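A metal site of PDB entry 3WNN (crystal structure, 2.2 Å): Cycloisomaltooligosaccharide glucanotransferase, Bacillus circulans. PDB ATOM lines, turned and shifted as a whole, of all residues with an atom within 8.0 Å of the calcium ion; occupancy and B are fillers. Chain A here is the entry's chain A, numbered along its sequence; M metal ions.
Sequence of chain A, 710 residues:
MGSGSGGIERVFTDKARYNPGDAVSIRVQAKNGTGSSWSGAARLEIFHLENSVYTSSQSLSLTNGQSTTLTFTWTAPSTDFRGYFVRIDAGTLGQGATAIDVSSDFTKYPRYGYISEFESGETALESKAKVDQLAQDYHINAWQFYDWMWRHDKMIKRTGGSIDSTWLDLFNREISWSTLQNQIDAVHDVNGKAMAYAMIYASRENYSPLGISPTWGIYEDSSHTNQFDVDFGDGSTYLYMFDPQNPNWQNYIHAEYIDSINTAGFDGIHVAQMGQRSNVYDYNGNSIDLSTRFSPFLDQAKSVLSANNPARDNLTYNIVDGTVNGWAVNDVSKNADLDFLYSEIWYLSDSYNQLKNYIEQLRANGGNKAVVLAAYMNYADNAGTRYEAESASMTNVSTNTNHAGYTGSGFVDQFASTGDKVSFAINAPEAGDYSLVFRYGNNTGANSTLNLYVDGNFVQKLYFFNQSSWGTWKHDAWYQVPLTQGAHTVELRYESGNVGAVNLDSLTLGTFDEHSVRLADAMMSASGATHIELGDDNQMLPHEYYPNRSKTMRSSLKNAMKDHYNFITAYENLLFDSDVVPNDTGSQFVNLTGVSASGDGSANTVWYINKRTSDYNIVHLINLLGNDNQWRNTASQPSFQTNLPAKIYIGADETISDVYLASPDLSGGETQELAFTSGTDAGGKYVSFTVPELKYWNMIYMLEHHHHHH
The backbone NH of Ser 409 lies close to the side-chain carboxylate of Glu 390, at 3.2 Å.
N of Gly 408 sits at hydrogen-bond distance from OE2 of Glu 388 (3.4 Å).
The backbone NH of Ala 389 sits close to the backbone carbonyl oxygen of Asp 505.
The guanidinium group of Arg 439 lies within salt-bridge range of the side-chain carboxylate of Asp 505 (2.9 Å).
OE2 of Glu 388 lies within salt-bridge range of NE of Arg 386 (3.3 Å).
Within 4 Å of the calcium ion: Glu 388, Glu 390, Thr 407, Gly 410 and Asp 505.
The calcium ion is bound by OD1 of Asp 505, O of Thr 407, O of Gly 410, OE1 of Glu 388, OE1 of Glu 390, O of Asp 505 and OE2 of Glu 390.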
ATOM      1  N   ARG A 386       5.226 -34.756   5.364  1.00  0.00           N
ATOM      2  CA  ARG A 386       5.979 -33.832   6.200  1.00  0.00           C
ATOM      3  C   ARG A 386       7.418 -33.672   5.713  1.00  0.00           C
ATOM      4  O   ARG A 386       8.103 -34.657   5.486  1.00  0.00           O
ATOM      5  CB  ARG A 386       6.015 -34.331   7.653  1.00  0.00           C
ATOM      6  CG  ARG A 386       6.548 -33.307   8.641  1.00  0.00           C
ATOM      7  CD  ARG A 386       6.000 -33.557  10.045  1.00  0.00           C
ATOM      8  NE  ARG A 386       6.370 -34.880  10.542  1.00  0.00           N
ATOM      9  CZ  ARG A 386       5.636 -35.678  11.329  1.00  0.00           C
ATOM     10  NH1 ARG A 386       4.421 -35.343  11.743  1.00  0.00           N
ATOM     11  NH2 ARG A 386       6.140 -36.844  11.702  1.00  0.00           N
ATOM     12  N   TYR A 387       7.853 -32.433   5.578  1.00  0.00           N
ATOM     13  CA  TYR A 387       9.259 -32.131   5.372  1.00  0.00           C
ATOM     14  C   TYR A 387       9.740 -31.466   6.635  1.00  0.00           C
ATOM     15  O   TYR A 387       9.341 -30.353   6.922  1.00  0.00           O
ATOM     16  CB  TYR A 387       9.451 -31.185   4.175  1.00  0.00           C
ATOM     17  CG  TYR A 387       9.005 -31.791   2.848  1.00  0.00           C
ATOM     18  CD1 TYR A 387       7.689 -31.721   2.415  1.00  0.00           C
ATOM     19  CD2 TYR A 387       9.930 -32.448   2.035  1.00  0.00           C
ATOM     20  CE1 TYR A 387       7.308 -32.294   1.199  1.00  0.00           C
ATOM     21  CE2 TYR A 387       9.546 -33.010   0.827  1.00  0.00           C
ATOM     22  CZ  TYR A 387       8.248 -32.939   0.408  1.00  0.00           C
ATOM     23  OH  TYR A 387       7.923 -33.504  -0.816  1.00  0.00           O
ATOM     24  N   GLU A 388      10.560 -32.178   7.399  1.00  0.00           N
ATOM     25  CA  GLU A 388      11.111 -31.687   8.653  1.00  0.00           C
ATOM     26  C   GLU A 388      11.998 -30.497   8.360  1.00  0.00           C
ATOM     27  O   GLU A 388      12.677 -30.485   7.366  1.00  0.00           O
ATOM     28  CB  GLU A 388      11.911 -32.800   9.348  1.00  0.00           C
ATOM     29  CG  GLU A 388      11.072 -33.959   9.895  1.00  0.00           C
ATOM     30  CD  GLU A 388      10.208 -33.575  11.108  1.00  0.00           C
ATOM     31  OE1 GLU A 388      10.287 -32.402  11.562  1.00  0.00           O
ATOM     32  OE2 GLU A 388       9.450 -34.435  11.628  1.00  0.00           O
ATOM     33  N   ALA A 389      11.959 -29.471   9.210  1.00  0.00           N
ATOM     34  CA  ALA A 389      12.705 -28.228   8.986  1.00  0.00           C
ATOM     35  C   ALA A 389      14.228 -28.389   9.176  1.00  0.00           C
ATOM     36  O   ALA A 389      15.042 -27.724   8.524  1.00  0.00           O
ATOM     37  CB  ALA A 389      12.174 -27.154   9.895  1.00  0.00           C
ATOM     38  N   GLU A 390      14.595 -29.252  10.103  1.00  0.00           N
ATOM     39  CA  GLU A 390      15.970 -29.590  10.371  1.00  0.00           C
ATOM     40  C   GLU A 390      16.594 -30.482   9.287  1.00  0.00           C
ATOM     41  O   GLU A 390      17.796 -30.694   9.293  1.00  0.00           O
ATOM     42  CB  GLU A 390      16.052 -30.314  11.701  1.00  0.00           C
ATOM     43  CG  GLU A 390      15.268 -31.636  11.741  1.00  0.00           C
ATOM     44  CD  GLU A 390      13.865 -31.534  12.369  1.00  0.00           C
ATOM     45  OE1 GLU A 390      13.193 -30.470  12.235  1.00  0.00           O
ATOM     46  OE2 GLU A 390      13.418 -32.536  12.978  1.00  0.00           O
ATOM     47  N   SER A 391      15.773 -31.034   8.389  1.00  0.00           N
ATOM     48  CA  SER A 391      16.279 -31.777   7.253  1.00  0.00           C
ATOM     49  C   SER A 391      16.207 -30.923   5.993  1.00  0.00           C
ATOM     50  O   SER A 391      16.378 -31.431   4.898  1.00  0.00           O
ATOM     51  CB  SER A 391      15.512 -33.099   7.085  1.00  0.00           C
ATOM     52  OG  SER A 391      15.330 -33.739   8.352  1.00  0.00           O
ATOM     53  N   ASN A 400      18.144 -27.400  16.938  1.00  0.00           N
ATOM     54  CA  ASN A 400      18.125 -27.412  18.405  1.00  0.00           C
ATOM     55  C   ASN A 400      17.117 -28.438  18.864  1.00  0.00           C
ATOM     56  O   ASN A 400      16.413 -28.987  18.034  1.00  0.00           O
ATOM     57  CB  ASN A 400      17.772 -26.025  18.956  1.00  0.00           C
ATOM     58  CG  ASN A 400      18.425 -25.748  20.303  1.00  0.00           C
ATOM     59  OD1 ASN A 400      18.675 -26.669  21.081  1.00  0.00           O
ATOM     60  ND2 ASN A 400      18.695 -24.472  20.587  1.00  0.00           N
ATOM     61  N   GLY A 405       8.126 -31.828  22.493  1.00  0.00           N
ATOM     62  CA  GLY A 405       7.004 -31.997  21.565  1.00  0.00           C
ATOM     63  C   GLY A 405       7.291 -31.848  20.075  1.00  0.00           C
ATOM     64  O   GLY A 405       6.450 -32.214  19.250  1.00  0.00           O
ATOM     65  N   TYR A 406       8.453 -31.303  19.707  1.00  0.00           N
ATOM     66  CA  TYR A 406       8.852 -31.219  18.311  1.00  0.00           C
ATOM     67  C   TYR A 406       8.802 -32.623  17.684  1.00  0.00           C
ATOM     68  O   TYR A 406       8.958 -33.633  18.380  1.00  0.00           O
ATOM     69  CB  TYR A 406      10.263 -30.618  18.158  1.00  0.00           C
ATOM     70  CG  TYR A 406      11.366 -31.423  18.834  1.00  0.00           C
ATOM     71  CD1 TYR A 406      11.815 -32.643  18.284  1.00  0.00           C
ATOM     72  CD2 TYR A 406      11.955 -30.973  20.024  1.00  0.00           C
ATOM     73  CE1 TYR A 406      12.818 -33.385  18.916  1.00  0.00           C
ATOM     74  CE2 TYR A 406      12.952 -31.713  20.663  1.00  0.00           C
ATOM     75  CZ  TYR A 406      13.376 -32.900  20.112  1.00  0.00           C
ATOM     76  OH  TYR A 406      14.370 -33.628  20.746  1.00  0.00           O
ATOM     77  N   THR A 407       8.520 -32.664  16.376  1.00  0.00           N
ATOM     78  CA  THR A 407       8.556 -33.909  15.600  1.00  0.00           C
ATOM     79  C   THR A 407       9.956 -34.088  14.975  1.00  0.00           C
ATOM     80  O   THR A 407      10.699 -33.120  14.680  1.00  0.00           O
ATOM     81  CB  THR A 407       7.541 -33.905  14.445  1.00  0.00           C
ATOM     82  OG1 THR A 407       7.933 -32.928  13.482  1.00  0.00           O
ATOM     83  CG2 THR A 407       6.125 -33.591  14.948  1.00  0.00           C
ATOM     84  N   GLY A 408      10.290 -35.346  14.745  1.00  0.00           N
ATOM     85  CA  GLY A 408      11.564 -35.716  14.151  1.00  0.00           C
ATOM     86  C   GLY A 408      12.678 -35.600  15.164  1.00  0.00           C
ATOM     87  O   GLY A 408      12.464 -35.817  16.362  1.00  0.00           O
ATOM     88  N   SER A 409      13.861 -35.246  14.673  1.00  0.00           N
ATOM     89  CA  SER A 409      15.081 -35.159  15.477  1.00  0.00           C
ATOM     90  C   SER A 409      15.247 -33.775  16.111  1.00  0.00           C
ATOM     91  O   SER A 409      16.032 -33.599  17.051  1.00  0.00           O
ATOM     92  CB  SER A 409      16.301 -35.407  14.589  1.00  0.00           C
ATOM     93  OG  SER A 409      16.574 -34.242  13.854  1.00  0.00           O
ATOM     94  N   GLY A 410      14.526 -32.790  15.602  1.00  0.00           N
ATOM     95  CA  GLY A 410      14.560 -31.481  16.250  1.00  0.00           C
ATOM     96  C   GLY A 410      13.712 -30.426  15.570  1.00  0.00           C
ATOM     97  O   GLY A 410      12.625 -30.705  15.074  1.00  0.00           O
ATOM     98  N   PHE A 411      14.216 -29.202  15.559  1.00  0.00           N
ATOM     99  CA  PHE A 411      13.543 -28.137  14.874  1.00  0.00           C
ATOM    100  C   PHE A 411      14.543 -27.013  14.688  1.00  0.00           C
ATOM    101  O   PHE A 411      15.581 -27.020  15.327  1.00  0.00           O
ATOM    102  CB  PHE A 411      12.387 -27.648  15.733  1.00  0.00           C
ATOM    103  CG  PHE A 411      12.808 -27.094  17.038  1.00  0.00           C
ATOM    104  CD1 PHE A 411      13.201 -25.760  17.149  1.00  0.00           C
ATOM    105  CD2 PHE A 411      12.809 -27.887  18.174  1.00  0.00           C
ATOM    106  CE1 PHE A 411      13.597 -25.228  18.372  1.00  0.00           C
ATOM    107  CE2 PHE A 411      13.200 -27.363  19.397  1.00  0.00           C
ATOM    108  CZ  PHE A 411      13.600 -26.031  19.499  1.00  0.00           C
ATOM    109  N   VAL A 412      14.227 -26.058  13.796  1.00  0.00           N
ATOM    110  CA  VAL A 412      15.066 -24.891  13.586  1.00  0.00           C
ATOM    111  C   VAL A 412      14.674 -23.777  14.547  1.00  0.00           C
ATOM    112  O   VAL A 412      13.511 -23.494  14.701  1.00  0.00           O
ATOM    113  CB  VAL A 412      14.962 -24.383  12.130  1.00  0.00           C
ATOM    114  CG1 VAL A 412      15.592 -22.997  11.976  1.00  0.00           C
ATOM    115  CG2 VAL A 412      15.593 -25.397  11.184  1.00  0.00           C
ATOM    116  N   ARG A 439       4.361 -25.991  10.992  1.00  0.00           N
ATOM    117  CA  ARG A 439       4.310 -26.140  12.438  1.00  0.00           C
ATOM    118  C   ARG A 439       5.443 -25.355  13.119  1.00  0.00           C
ATOM    119  O   ARG A 439       6.607 -25.523  12.782  1.00  0.00           O
ATOM    120  CB  ARG A 439       4.425 -27.601  12.850  1.00  0.00           C
ATOM    121  CG  ARG A 439       4.083 -27.852  14.304  1.00  0.00           C
ATOM    122  CD  ARG A 439       4.094 -29.352  14.548  1.00  0.00           C
ATOM    123  NE  ARG A 439       3.464 -29.757  15.816  1.00  0.00           N
ATOM    124  CZ  ARG A 439       4.081 -30.212  16.906  1.00  0.00           C
ATOM    125  NH1 ARG A 439       5.399 -30.329  16.959  1.00  0.00           N
ATOM    126  NH2 ARG A 439       3.371 -30.571  17.954  1.00  0.00           N
ATOM    127  N   TRP A 473       3.419 -25.781  20.458  1.00  0.00           N
ATOM    128  CA  TRP A 473       3.468 -25.888  19.029  1.00  0.00           C
ATOM    129  C   TRP A 473       2.052 -25.674  18.443  1.00  0.00           C
ATOM    130  O   TRP A 473       1.104 -26.256  18.941  1.00  0.00           O
ATOM    131  CB  TRP A 473       4.003 -27.273  18.665  1.00  0.00           C
ATOM    132  CG  TRP A 473       5.391 -27.531  19.174  1.00  0.00           C
ATOM    133  CD1 TRP A 473       5.737 -28.373  20.184  1.00  0.00           C
ATOM    134  CD2 TRP A 473       6.618 -26.955  18.694  1.00  0.00           C
ATOM    135  NE1 TRP A 473       7.114 -28.367  20.361  1.00  0.00           N
ATOM    136  CE2 TRP A 473       7.669 -27.495  19.463  1.00  0.00           C
ATOM    137  CE3 TRP A 473       6.927 -26.031  17.676  1.00  0.00           C
ATOM    138  CZ2 TRP A 473       9.007 -27.150  19.245  1.00  0.00           C
ATOM    139  CZ3 TRP A 473       8.252 -25.683  17.473  1.00  0.00           C
ATOM    140  CH2 TRP A 473       9.268 -26.252  18.245  1.00  0.00           C
ATOM    141  N   LEU A 504      10.912 -23.338  14.080  1.00  0.00           N
ATOM    142  CA  LEU A 504      10.242 -23.971  12.957  1.00  0.00           C
ATOM    143  C   LEU A 504      10.449 -25.451  12.976  1.00  0.00           C
ATOM    144  O   LEU A 504      11.544 -25.922  12.809  1.00  0.00           O
ATOM    145  CB  LEU A 504      10.707 -23.392  11.607  1.00  0.00           C
ATOM    146  CG  LEU A 504       9.936 -23.872  10.354  1.00  0.00           C
ATOM    147  CD1 LEU A 504       8.527 -23.301  10.347  1.00  0.00           C
ATOM    148  CD2 LEU A 504      10.625 -23.468   9.056  1.00  0.00           C
ATOM    149  N   ASP A 505       9.377 -26.212  13.178  1.00  0.00           N
ATOM    150  CA  ASP A 505       9.476 -27.653  13.350  1.00  0.00           C
ATOM    151  C   ASP A 505       9.452 -28.424  11.998  1.00  0.00           C
ATOM    152  O   ASP A 505      10.194 -29.430  11.809  1.00  0.00           O
ATOM    153  CB  ASP A 505       8.379 -28.197  14.281  1.00  0.00           C
ATOM    154  CG  ASP A 505       8.650 -29.610  14.717  1.00  0.00           C
ATOM    155  OD1 ASP A 505       9.826 -30.016  14.536  1.00  0.00           O
ATOM    156  OD2 ASP A 505       7.741 -30.334  15.227  1.00  0.00           O
ATOM    157  N   SER A 506       8.626 -27.953  11.075  1.00  0.00           N
ATOM    158  CA  SER A 506       8.352 -28.709   9.869  1.00  0.00           C
ATOM    159  C   SER A 506       7.443 -27.937   8.967  1.00  0.00           C
ATOM    160  O   SER A 506       6.790 -27.022   9.433  1.00  0.00           O
ATOM    161  CB  SER A 506       7.675 -30.066  10.201  1.00  0.00           C
ATOM    162  OG  SER A 506       6.481 -29.918  10.937  1.00  0.00           O
ATOM    163  N   LEU A 507       7.445 -28.310   7.691  1.00  0.00           N
ATOM    164  CA  LEU A 507       6.449 -27.928   6.688  1.00  0.00           C
ATOM    165  C   LEU A 507       5.678 -29.200   6.335  1.00  0.00           C
ATOM    166  O   LEU A 507       6.275 -30.273   6.226  1.00  0.00           O
ATOM    167  CB  LEU A 507       7.146 -27.418   5.399  1.00  0.00           C
ATOM    168  CG  LEU A 507       6.343 -27.353   4.075  1.00  0.00           C
ATOM    169  CD1 LEU A 507       5.112 -26.465   4.154  1.00  0.00           C
ATOM    170  CD2 LEU A 507       7.203 -26.892   2.916  1.00  0.00           C
HETATM  171 CA    CA M   1      11.095 -31.249  13.413  1.00  0.00          CA
